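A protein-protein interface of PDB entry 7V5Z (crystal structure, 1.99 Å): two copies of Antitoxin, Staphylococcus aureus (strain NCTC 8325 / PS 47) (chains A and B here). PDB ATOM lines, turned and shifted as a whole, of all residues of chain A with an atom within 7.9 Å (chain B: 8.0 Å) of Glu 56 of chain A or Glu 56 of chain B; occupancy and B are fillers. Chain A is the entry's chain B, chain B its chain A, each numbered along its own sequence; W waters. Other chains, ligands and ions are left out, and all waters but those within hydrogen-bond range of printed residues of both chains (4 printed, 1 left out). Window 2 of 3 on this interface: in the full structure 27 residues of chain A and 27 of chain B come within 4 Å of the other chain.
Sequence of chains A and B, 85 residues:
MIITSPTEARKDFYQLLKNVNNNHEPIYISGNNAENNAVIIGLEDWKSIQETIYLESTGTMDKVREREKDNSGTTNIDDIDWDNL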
ATOM      1  N   ILE A  49     -14.316   4.046 -19.996  1.00  0.00           N
ATOM      2  CA  ILE A  49     -13.557   5.136 -19.407  1.00  0.00           C
ATOM      3  C   ILE A  49     -13.137   6.123 -20.486  1.00  0.00           C
ATOM      4  O   ILE A  49     -13.278   7.344 -20.333  1.00  0.00           O
ATOM      5  CB  ILE A  49     -12.343   4.586 -18.642  1.00  0.00           C
ATOM      6  CG1 ILE A  49     -12.792   3.887 -17.348  1.00  0.00           C
ATOM      7  CG2 ILE A  49     -11.335   5.689 -18.404  1.00  0.00           C
ATOM      8  CD1 ILE A  49     -11.669   3.100 -16.663  1.00  0.00           C
ATOM      9  N   GLN A  50     -12.589   5.608 -21.590  1.00  0.00           N
ATOM     10  CA  GLN A  50     -12.076   6.504 -22.616  1.00  0.00           C
ATOM     11  C   GLN A  50     -13.209   7.301 -23.235  1.00  0.00           C
ATOM     12  O   GLN A  50     -13.067   8.500 -23.495  1.00  0.00           O
ATOM     13  CB  GLN A  50     -11.313   5.709 -23.680  1.00  0.00           C
ATOM     14  CG  GLN A  50      -9.996   5.110 -23.165  1.00  0.00           C
ATOM     15  CD  GLN A  50      -9.033   6.176 -22.627  1.00  0.00           C
ATOM     16  OE1 GLN A  50      -8.890   7.247 -23.218  1.00  0.00           O
ATOM     17  NE2 GLN A  50      -8.375   5.883 -21.509  1.00  0.00           N
ATOM     18  N   GLU A  51     -14.355   6.656 -23.453  1.00  0.00           N
ATOM     19  CA  GLU A  51     -15.492   7.377 -24.016  1.00  0.00           C
ATOM     20  C   GLU A  51     -15.988   8.449 -23.053  1.00  0.00           C
ATOM     21  O   GLU A  51     -16.417   9.527 -23.482  1.00  0.00           O
ATOM     22  CB  GLU A  51     -16.610   6.399 -24.379  1.00  0.00           C
ATOM     23  CG  GLU A  51     -17.929   7.051 -24.733  1.00  0.00           C
ATOM     24  CD  GLU A  51     -17.978   7.528 -26.181  1.00  0.00           C
ATOM     25  OE1 GLU A  51     -16.953   7.412 -26.899  1.00  0.00           O
ATOM     26  OE2 GLU A  51     -19.044   8.018 -26.594  1.00  0.00           O
ATOM     27  N   THR A  52     -15.921   8.183 -21.747  1.00  0.00           N
ATOM     28  CA  THR A  52     -16.339   9.189 -20.774  1.00  0.00           C
ATOM     29  C   THR A  52     -15.409  10.391 -20.794  1.00  0.00           C
ATOM     30  O   THR A  52     -15.862  11.543 -20.784  1.00  0.00           O
ATOM     31  CB  THR A  52     -16.388   8.588 -19.362  1.00  0.00           C
ATOM     32  OG1 THR A  52     -17.343   7.532 -19.340  1.00  0.00           O
ATOM     33  CG2 THR A  52     -16.832   9.652 -18.356  1.00  0.00           C
ATOM     34  N   ILE A  53     -14.097  10.145 -20.782  1.00  0.00           N
ATOM     35  CA  ILE A  53     -13.138  11.248 -20.779  1.00  0.00           C
ATOM     36  C   ILE A  53     -13.301  12.104 -22.035  1.00  0.00           C
ATOM     37  O   ILE A  53     -13.259  13.339 -21.971  1.00  0.00           O
ATOM     38  CB  ILE A  53     -11.705  10.707 -20.618  1.00  0.00           C
ATOM     39  CG1 ILE A  53     -11.489  10.207 -19.185  1.00  0.00           C
ATOM     40  CG2 ILE A  53     -10.683  11.773 -20.923  1.00  0.00           C
ATOM     41  CD1 ILE A  53     -10.286   9.299 -19.059  1.00  0.00           C
ATOM     42  N   TYR A  54     -13.544  11.467 -23.183  1.00  0.00           N
ATOM     43  CA  TYR A  54     -13.729  12.219 -24.426  1.00  0.00           C
ATOM     44  C   TYR A  54     -14.977  13.091 -24.368  1.00  0.00           C
ATOM     45  O   TYR A  54     -14.930  14.290 -24.677  1.00  0.00           O
ATOM     46  CB  TYR A  54     -13.825  11.265 -25.620  1.00  0.00           C
ATOM     47  CG  TYR A  54     -14.365  11.940 -26.883  1.00  0.00           C
ATOM     48  CD1 TYR A  54     -13.627  12.934 -27.515  1.00  0.00           C
ATOM     49  CD2 TYR A  54     -15.615  11.598 -27.420  1.00  0.00           C
ATOM     50  CE1 TYR A  54     -14.088  13.560 -28.660  1.00  0.00           C
ATOM     51  CE2 TYR A  54     -16.106  12.235 -28.568  1.00  0.00           C
ATOM     52  CZ  TYR A  54     -15.322  13.220 -29.181  1.00  0.00           C
ATOM     53  OH  TYR A  54     -15.757  13.877 -30.318  1.00  0.00           O
ATOM     54  N   LEU A  55     -16.117  12.501 -24.015  1.00  0.00           N
ATOM     55  CA  LEU A  55     -17.337  13.298 -23.975  1.00  0.00           C
ATOM     56  C   LEU A  55     -17.271  14.357 -22.888  1.00  0.00           C
ATOM     57  O   LEU A  55     -17.821  15.449 -23.068  1.00  0.00           O
ATOM     58  CB  LEU A  55     -18.549  12.405 -23.765  1.00  0.00           C
ATOM     59  CG  LEU A  55     -18.946  11.530 -24.947  1.00  0.00           C
ATOM     60  CD1 LEU A  55     -20.136  10.653 -24.577  1.00  0.00           C
ATOM     61  CD2 LEU A  55     -19.247  12.400 -26.142  1.00  0.00           C
ATOM     62  N   GLU A  56     -16.596  14.073 -21.763  1.00  0.00           N
ATOM     63  CA  GLU A  56     -16.455  15.112 -20.746  1.00  0.00           C
ATOM     64  C   GLU A  56     -15.605  16.270 -21.255  1.00  0.00           C
ATOM     65  O   GLU A  56     -15.974  17.440 -21.079  1.00  0.00           O
ATOM     66  CB  GLU A  56     -15.856  14.544 -19.455  1.00  0.00           C
ATOM     67  CG  GLU A  56     -16.801  13.667 -18.629  1.00  0.00           C
ATOM     68  CD  GLU A  56     -17.959  14.433 -17.966  1.00  0.00           C
ATOM     69  OE1 GLU A  56     -18.065  15.670 -18.160  1.00  0.00           O
ATOM     70  OE2 GLU A  56     -18.781  13.786 -17.258  1.00  0.00           O
ATOM     71  N   SER A  57     -14.467  15.980 -21.894  1.00  0.00           N
ATOM     72  CA  SER A  57     -13.574  17.076 -22.267  1.00  0.00           C
ATOM     73  C   SER A  57     -14.112  17.906 -23.433  1.00  0.00           C
ATOM     74  O   SER A  57     -13.699  19.064 -23.597  1.00  0.00           O
ATOM     75  CB  SER A  57     -12.164  16.543 -22.582  1.00  0.00           C
ATOM     76  OG  SER A  57     -12.148  15.846 -23.817  1.00  0.00           O
ATOM     77  N   THR A  58     -15.035  17.367 -24.223  1.00  0.00           N
ATOM     78  CA  THR A  58     -15.677  18.158 -25.263  1.00  0.00           C
ATOM     79  C   THR A  58     -16.764  19.066 -24.714  1.00  0.00           C
ATOM     80  O   THR A  58     -17.355  19.830 -25.483  1.00  0.00           O
ATOM     81  CB  THR A  58     -16.301  17.268 -26.340  1.00  0.00           C
ATOM     82  OG1 THR A  58     -17.394  16.537 -25.780  1.00  0.00           O
ATOM     83  CG2 THR A  58     -15.287  16.322 -26.941  1.00  0.00           C
ATOM     84  N   GLY A  59     -17.052  18.985 -23.419  1.00  0.00           N
ATOM     85  CA  GLY A  59     -18.150  19.717 -22.843  1.00  0.00           C
ATOM     86  C   GLY A  59     -19.512  19.106 -23.086  1.00  0.00           C
ATOM     87  O   GLY A  59     -20.519  19.710 -22.698  1.00  0.00           O
ATOM     88  N   THR A  60     -19.578  17.936 -23.725  1.00  0.00           N
ATOM     89  CA  THR A  60     -20.872  17.323 -24.009  1.00  0.00           C
ATOM     90  C   THR A  60     -21.597  16.945 -22.726  1.00  0.00           C
ATOM     91  O   THR A  60     -22.799  17.191 -22.587  1.00  0.00           O
ATOM     92  CB  THR A  60     -20.690  16.092 -24.901  1.00  0.00           C
ATOM     93  OG1 THR A  60     -20.019  16.464 -26.107  1.00  0.00           O
ATOM     94  CG2 THR A  60     -22.036  15.463 -25.255  1.00  0.00           C
ATOM     95  N   MET A  61     -20.894  16.333 -21.779  1.00  0.00           N
ATOM     96  CA  MET A  61     -21.585  15.900 -20.570  1.00  0.00           C
ATOM     97  C   MET A  61     -22.004  17.082 -19.712  1.00  0.00           C
ATOM     98  O   MET A  61     -23.000  16.987 -18.990  1.00  0.00           O
ATOM     99  CB  MET A  61     -20.707  14.926 -19.784  1.00  0.00           C
ATOM    100  CG  MET A  61     -20.372  13.648 -20.577  1.00  0.00           C
ATOM    101  SD  MET A  61     -21.857  12.861 -21.280  1.00  0.00           S
ATOM    102  CE  MET A  61     -22.771  12.444 -19.785  1.00  0.00           C
ATOM    103  N   ASP A  62     -21.272  18.202 -19.786  1.00  0.00           N
ATOM    104  CA  ASP A  62     -21.731  19.435 -19.144  1.00  0.00           C
ATOM    105  C   ASP A  62     -23.068  19.868 -19.718  1.00  0.00           C
ATOM    106  O   ASP A  62     -23.995  20.230 -18.982  1.00  0.00           O
ATOM    107  CB  ASP A  62     -20.708  20.563 -19.344  1.00  0.00           C
ATOM    108  CG  ASP A  62     -19.392  20.307 -18.646  1.00  0.00           C
ATOM    109  OD1 ASP A  62     -19.311  19.364 -17.835  1.00  0.00           O
ATOM    110  OD2 ASP A  62     -18.431  21.065 -18.915  1.00  0.00           O
ATOM    111  N   LYS A  63     -23.163  19.872 -21.049  1.00  0.00           N
ATOM    112  CA  LYS A  63     -24.401  20.224 -21.727  1.00  0.00           C
ATOM    113  C   LYS A  63     -25.520  19.259 -21.350  1.00  0.00           C
ATOM    114  O   LYS A  63     -26.656  19.681 -21.084  1.00  0.00           O
ATOM    115  CB  LYS A  63     -24.139  20.240 -23.244  1.00  0.00           C
ATOM    116  CG  LYS A  63     -25.263  20.757 -24.123  1.00  0.00           C
ATOM    117  CD  LYS A  63     -24.802  20.832 -25.606  1.00  0.00           C
ATOM    118  CE  LYS A  63     -24.433  19.476 -26.210  1.00  0.00           C
ATOM    119  NZ  LYS A  63     -24.372  19.574 -27.737  1.00  0.00           N
ATOM    120  N   ARG A  65     -25.813  17.368 -18.516  1.00  0.00           N
ATOM    121  CA  ARG A  65     -26.246  17.568 -17.131  1.00  0.00           C
ATOM    122  C   ARG A  65     -27.086  18.828 -16.976  1.00  0.00           C
ATOM    123  O   ARG A  65     -28.000  18.865 -16.147  1.00  0.00           O
ATOM    124  CB  ARG A  65     -25.042  17.631 -16.179  1.00  0.00           C
ATOM    125  CG  ARG A  65     -24.430  16.257 -15.792  1.00  0.00           C
ATOM    126  CD  ARG A  65     -23.202  16.411 -14.874  1.00  0.00           C
ATOM    127  NE  ARG A  65     -22.062  17.037 -15.555  1.00  0.00           N
ATOM    128  CZ  ARG A  65     -21.068  16.362 -16.129  1.00  0.00           C
ATOM    129  NH1 ARG A  65     -21.061  15.033 -16.100  1.00  0.00           N
ATOM    130  NH2 ARG A  65     -20.080  17.009 -16.738  1.00  0.00           N
ATOM    131  N   ILE B  49      -6.093   8.559 -14.499  1.00  0.00           N
ATOM    132  CA  ILE B  49      -7.408   8.244 -15.043  1.00  0.00           C
ATOM    133  C   ILE B  49      -8.426   8.105 -13.921  1.00  0.00           C
ATOM    134  O   ILE B  49      -9.528   8.654 -13.996  1.00  0.00           O
ATOM    135  CB  ILE B  49      -7.324   6.969 -15.901  1.00  0.00           C
ATOM    136  CG1 ILE B  49      -6.630   7.290 -17.227  1.00  0.00           C
ATOM    137  CG2 ILE B  49      -8.712   6.374 -16.110  1.00  0.00           C
ATOM    138  CD1 ILE B  49      -5.799   6.159 -17.766  1.00  0.00           C
ATOM    139  N   GLN B  50      -8.070   7.367 -12.862  1.00  0.00           N
ATOM    140  CA  GLN B  50      -8.957   7.213 -11.712  1.00  0.00           C
ATOM    141  C   GLN B  50      -9.331   8.562 -11.115  1.00  0.00           C
ATOM    142  O   GLN B  50     -10.487   8.795 -10.740  1.00  0.00           O
ATOM    143  CB  GLN B  50      -8.278   6.370 -10.636  1.00  0.00           C
ATOM    144  CG  GLN B  50      -8.553   4.878 -10.682  1.00  0.00           C
ATOM    145  CD  GLN B  50      -7.909   4.170  -9.497  1.00  0.00           C
ATOM    146  OE1 GLN B  50      -6.892   4.634  -8.964  1.00  0.00           O
ATOM    147  NE2 GLN B  50      -8.493   3.048  -9.078  1.00  0.00           N
ATOM    148  N   GLU B  51      -8.352   9.441 -10.972  1.00  0.00           N
ATOM    149  CA  GLU B  51      -8.621  10.749 -10.392  1.00  0.00           C
ATOM    150  C   GLU B  51      -9.502  11.589 -11.316  1.00  0.00           C
ATOM    151  O   GLU B  51     -10.405  12.296 -10.853  1.00  0.00           O
ATOM    152  CB  GLU B  51      -7.295  11.452 -10.096  1.00  0.00           C
ATOM    153  CG  GLU B  51      -7.449  12.887  -9.603  1.00  0.00           C
ATOM    154  CD  GLU B  51      -7.976  13.006  -8.172  1.00  0.00           C
ATOM    155  OE1 GLU B  51      -8.306  11.976  -7.545  1.00  0.00           O
ATOM    156  OE2 GLU B  51      -8.056  14.152  -7.672  1.00  0.00           O
ATOM    157  N   THR B  52      -9.261  11.517 -12.625  1.00  0.00           N
ATOM    158  CA  THR B  52     -10.086  12.247 -13.579  1.00  0.00           C
ATOM    159  C   THR B  52     -11.531  11.771 -13.540  1.00  0.00           C
ATOM    160  O   THR B  52     -12.471  12.579 -13.530  1.00  0.00           O
ATOM    161  CB  THR B  52      -9.526  12.075 -14.988  1.00  0.00           C
ATOM    162  OG1 THR B  52      -8.200  12.603 -15.033  1.00  0.00           O
ATOM    163  CG2 THR B  52     -10.417  12.815 -16.003  1.00  0.00           C
ATOM    164  N   ILE B  53     -11.728  10.455 -13.541  1.00  0.00           N
ATOM    165  CA  ILE B  53     -13.082   9.909 -13.501  1.00  0.00           C
ATOM    166  C   ILE B  53     -13.789  10.363 -12.227  1.00  0.00           C
ATOM    167  O   ILE B  53     -14.976  10.699 -12.244  1.00  0.00           O
ATOM    168  CB  ILE B  53     -13.047   8.369 -13.627  1.00  0.00           C
ATOM    169  CG1 ILE B  53     -12.620   7.932 -15.035  1.00  0.00           C
ATOM    170  CG2 ILE B  53     -14.403   7.722 -13.231  1.00  0.00           C
ATOM    171  CD1 ILE B  53     -13.558   8.367 -16.150  1.00  0.00           C
ATOM    172  N   TYR B  54     -13.066  10.413 -11.112  1.00  0.00           N
ATOM    173  CA  TYR B  54     -13.683  10.864  -9.865  1.00  0.00           C
ATOM    174  C   TYR B  54     -14.102  12.332  -9.947  1.00  0.00           C
ATOM    175  O   TYR B  54     -15.217  12.684  -9.553  1.00  0.00           O
ATOM    176  CB  TYR B  54     -12.731  10.648  -8.692  1.00  0.00           C
ATOM    177  CG  TYR B  54     -13.223  11.301  -7.410  1.00  0.00           C
ATOM    178  CD1 TYR B  54     -14.276  10.761  -6.693  1.00  0.00           C
ATOM    179  CD2 TYR B  54     -12.634  12.475  -6.930  1.00  0.00           C
ATOM    180  CE1 TYR B  54     -14.730  11.369  -5.514  1.00  0.00           C
ATOM    181  CE2 TYR B  54     -13.085  13.092  -5.747  1.00  0.00           C
ATOM    182  CZ  TYR B  54     -14.130  12.529  -5.052  1.00  0.00           C
ATOM    183  OH  TYR B  54     -14.578  13.128  -3.896  1.00  0.00           O
ATOM    184  N   LEU B  55     -13.220  13.209 -10.445  1.00  0.00           N
ATOM    185  CA  LEU B  55     -13.590  14.623 -10.536  1.00  0.00           C
ATOM    186  C   LEU B  55     -14.648  14.882 -11.615  1.00  0.00           C
ATOM    187  O   LEU B  55     -15.418  15.845 -11.506  1.00  0.00           O
ATOM    188  CB  LEU B  55     -12.347  15.484 -10.771  1.00  0.00           C
ATOM    189  CG  LEU B  55     -11.321  15.415  -9.621  1.00  0.00           C
ATOM    190  CD1 LEU B  55      -9.982  16.144  -9.958  1.00  0.00           C
ATOM    191  CD2 LEU B  55     -11.930  15.969  -8.347  1.00  0.00           C
ATOM    192  N   GLU B  56     -14.718  14.048 -12.656  1.00  0.00           N
ATOM    193  CA  GLU B  56     -15.829  14.187 -13.599  1.00  0.00           C
ATOM    194  C   GLU B  56     -17.127  13.658 -13.001  1.00  0.00           C
ATOM    195  O   GLU B  56     -18.192  14.259 -13.188  1.00  0.00           O
ATOM    196  CB  GLU B  56     -15.530  13.462 -14.915  1.00  0.00           C
ATOM    197  CG  GLU B  56     -14.310  13.983 -15.664  1.00  0.00           C
ATOM    198  CD  GLU B  56     -14.539  15.300 -16.372  1.00  0.00           C
ATOM    199  OE1 GLU B  56     -15.656  15.866 -16.286  1.00  0.00           O
ATOM    200  OE2 GLU B  56     -13.580  15.786 -17.014  1.00  0.00           O
ATOM    201  N   SER B  57     -17.061  12.540 -12.280  1.00  0.00           N
ATOM    202  CA  SER B  57     -18.284  11.917 -11.767  1.00  0.00           C
ATOM    203  C   SER B  57     -18.947  12.767 -10.696  1.00  0.00           C
ATOM    204  O   SER B  57     -20.166  12.687 -10.507  1.00  0.00           O
ATOM    205  CB  SER B  57     -17.974  10.526 -11.216  1.00  0.00           C
ATOM    206  OG  SER B  57     -17.625   9.651 -12.280  1.00  0.00           O
ATOM    207  N   THR B  58     -18.172  13.580  -9.981  1.00  0.00           N
ATOM    208  CA  THR B  58     -18.768  14.447  -8.978  1.00  0.00           C
ATOM    209  C   THR B  58     -19.273  15.758  -9.563  1.00  0.00           C
ATOM    210  O   THR B  58     -19.873  16.559  -8.835  1.00  0.00           O
ATOM    211  CB  THR B  58     -17.759  14.728  -7.858  1.00  0.00           C
ATOM    212  OG1 THR B  58     -16.592  15.367  -8.393  1.00  0.00           O
ATOM    213  CG2 THR B  58     -17.341  13.428  -7.176  1.00  0.00           C
ATOM    214  N   GLY B  59     -19.058  16.003 -10.851  1.00  0.00           N
ATOM    215  CA  GLY B  59     -19.349  17.309 -11.400  1.00  0.00           C
ATOM    216  C   GLY B  59     -18.290  18.363 -11.170  1.00  0.00           C
ATOM    217  O   GLY B  59     -18.499  19.520 -11.551  1.00  0.00           O
ATOM    218  N   THR B  60     -17.153  18.004 -10.573  1.00  0.00           N
ATOM    219  CA  THR B  60     -16.135  19.003 -10.268  1.00  0.00           C
ATOM    220  C   THR B  60     -15.521  19.583 -11.536  1.00  0.00           C
ATOM    221  O   THR B  60     -15.325  20.800 -11.629  1.00  0.00           O
ATOM    222  CB  THR B  60     -15.058  18.391  -9.365  1.00  0.00           C
ATOM    223  OG1 THR B  60     -15.672  17.956  -8.140  1.00  0.00           O
ATOM    224  CG2 THR B  60     -13.974  19.420  -9.054  1.00  0.00           C
ATOM    225  N   MET B  61     -15.215  18.732 -12.528  1.00  0.00           N
ATOM    226  CA  MET B  61     -14.621  19.227 -13.768  1.00  0.00           C
ATOM    227  C   MET B  61     -15.625  20.053 -14.564  1.00  0.00           C
ATOM    228  O   MET B  61     -15.242  21.001 -15.256  1.00  0.00           O
ATOM    229  CB  MET B  61     -14.093  18.055 -14.616  1.00  0.00           C
ATOM    230  CG  MET B  61     -12.922  17.290 -14.016  1.00  0.00           C
ATOM    231  SD  MET B  61     -11.728  18.375 -13.169  1.00  0.00           S
ATOM    232  CE  MET B  61     -10.955  19.173 -14.580  1.00  0.00           C
ATOM    233  N   ASP B  62     -16.909  19.712 -14.461  1.00  0.00           N
ATOM    234  CA  ASP B  62     -17.976  20.548 -15.001  1.00  0.00           C
ATOM    235  C   ASP B  62     -17.881  21.975 -14.464  1.00  0.00           C
ATOM    236  O   ASP B  62     -17.912  22.947 -15.225  1.00  0.00           O
ATOM    237  CB  ASP B  62     -19.324  19.895 -14.649  1.00  0.00           C
ATOM    238  CG  ASP B  62     -20.527  20.576 -15.295  1.00  0.00           C
ATOM    239  OD1 ASP B  62     -20.482  21.786 -15.603  1.00  0.00           O
ATOM    240  OD2 ASP B  62     -21.555  19.879 -15.461  1.00  0.00           O
ATOM    241  N   LYS B  63     -17.757  22.118 -13.147  1.00  0.00           N
ATOM    242  CA  LYS B  63     -17.655  23.452 -12.574  1.00  0.00           C
ATOM    243  C   LYS B  63     -16.315  24.104 -12.905  1.00  0.00           C
ATOM    244  O   LYS B  63     -16.255  25.314 -13.159  1.00  0.00           O
ATOM    245  CB  LYS B  63     -17.872  23.392 -11.062  1.00  0.00           C
ATOM    246  CG  LYS B  63     -18.002  24.785 -10.456  1.00  0.00           C
ATOM    247  CD  LYS B  63     -18.278  24.724  -8.959  1.00  0.00           C
ATOM    248  CE  LYS B  63     -19.454  23.833  -8.614  1.00  0.00           C
ATOM    249  NZ  LYS B  63     -19.016  22.596  -7.905  1.00  0.00           N
ATOM    250  N   ARG B  65     -14.558  23.717 -15.667  1.00  0.00           N
ATOM    251  CA  ARG B  65     -14.619  24.198 -17.047  1.00  0.00           C
ATOM    252  C   ARG B  65     -15.444  25.474 -17.154  1.00  0.00           C
ATOM    253  O   ARG B  65     -15.087  26.390 -17.904  1.00  0.00           O
ATOM    254  CB  ARG B  65     -15.187  23.108 -17.963  1.00  0.00           C
ATOM    255  CG  ARG B  65     -14.168  22.041 -18.347  1.00  0.00           C
ATOM    256  CD  ARG B  65     -14.751  20.985 -19.324  1.00  0.00           C
ATOM    257  NE  ARG B  65     -15.752  20.121 -18.699  1.00  0.00           N
ATOM    258  CZ  ARG B  65     -15.486  18.928 -18.164  1.00  0.00           C
ATOM    259  NH1 ARG B  65     -14.245  18.445 -18.163  1.00  0.00           N
ATOM    260  NH2 ARG B  65     -16.458  18.219 -17.615  1.00  0.00           N
HETATM  261  O   HOH W   1     -17.615  16.900 -14.426  1.00  0.00           O
HETATM  262  O   HOH W   2     -23.568  21.311 -16.483  1.00  0.00           O
HETATM  263  O   HOH W   3     -19.044  23.537 -17.572  1.00  0.00           O
HETATM  264  O   HOH W   4     -12.296  14.699 -19.406  1.00  0.00           O
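Among the printed residues, merely in contact across the chains: Ile 49 of chain A with Ile 49 of chain B (3.6 Å) and Arg 65 of chain A with Arg 65 of chain B (3.9 Å).
The guanidinium group (NH2) of Arg 65 of chain B lies within salt-bridge range of the side-chain carboxylate (OE1) of Glu 56 of chain B (2.8 Å).
OE1 of Glu 56 of chain A is in salt-bridge range of NH2 of Arg 65 of chain A (2.8 Å).
OD1 of Asp 62 of chain A is in salt-bridge range of NH2 of Arg 65 of chain A (2.7 Å).
Water W3 lies within hydrogen-bond range of the backbone carbonyl oxygen of Asp 62 of chain B (2.7 Å) and the side-chain carboxylate of Asp 62 of chain A (2.9 Å).
Water W2 lies within hydrogen-bond range of the side-chain carboxylate (OD2) of Asp 62 of chain B (2.7 Å) and the backbone carbonyl oxygen (O) of Asp 62 of chain A (2.8 Å).
Water W1 lies within hydrogen-bond range of OE1 of Glu 56 of chain B (2.9 Å), N of Asp 62 of chain B (2.9 Å) and NH2 of Arg 65 of chain A (3.4 Å).
Water W4 bridges OE2 of Glu 56 of chain B and O of Ile 53 of chain A.
Of the printed residues of chain B, Ile 49 of chain A touches Ile 49.
Glu 51 of chain A touches none of the printed residues of chain B.
Of the printed residues of chain A, Ile 49 of chain B touches Ile 49 (3.6 Å).
Glu 56 of chain B touches just one residue of chain A: Glu 56.
Of the printed residues of chain A, Asp 62 of chain B touches Asp 62 (3.1 Å) and Arg 65 (2.9 Å).
Printed residues of chain A within 4 Å of Arg 65 of chain B: Glu 56 (3.1 Å), Asp 62 (2.8 Å) and Arg 65 (3.9 Å).
The nearest residue of chain B that does not touch Glu 56 of chain A is Ser 57 of chain B (5.4 Å).
Printed residues of chain A that touch a printed residue of chain B: Ile 49, Glu 56, Asp 62 and Arg 65.
Hydrophobic or aromatic side chains of chain A that line the printed part of chain B: Ile 49.
Of the 16 printed residues of chain B, 4 touch a printed residue of chain A.
Hydrophobic or aromatic side chains of chain B within 4 Å of the printed part of chain A: Ile 49.
Ile 49 of chain A touches its own counterpart, Ile 49 of chain B.
Glu 56 of chain A touches its own counterpart, Glu 56 of chain B.
Glu 56 of chain A touches Arg 65 of chain B, but with the chains exchanged Arg 65 of chain A does not touch Glu 56 of chain B (4.2 Å).
Asp 62 of chain A touches its own counterpart, Asp 62 of chain B.
Positions printed for both chains: 49, 50, 51, 52, 53, 54, 55, 56, 57, 58, 59, 60, 61, 62, 63 and 65.
The guanidinium group of Arg 65 of chain A is in salt-bridge range of the side-chain carboxylate of Asp 62 of chain B (2.9 Å).
The guanidinium group of Arg 65 of chain B is in salt-bridge range of the side-chain carboxylate of Glu 56 of chain A (3.1 Å).
OD2 of Asp 62 of chain A is in salt-bridge range of NE of Arg 65 of chain B.
OE1 of Glu 56 of chain B lies close to OE1 of Glu 56 of chain A (3.1 Å).
The side-chain carboxylate (OD1) of Asp 62 of chain A sits close to the side-chain carboxylate (OD2) of Asp 62 of chain B (3.3 Å).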
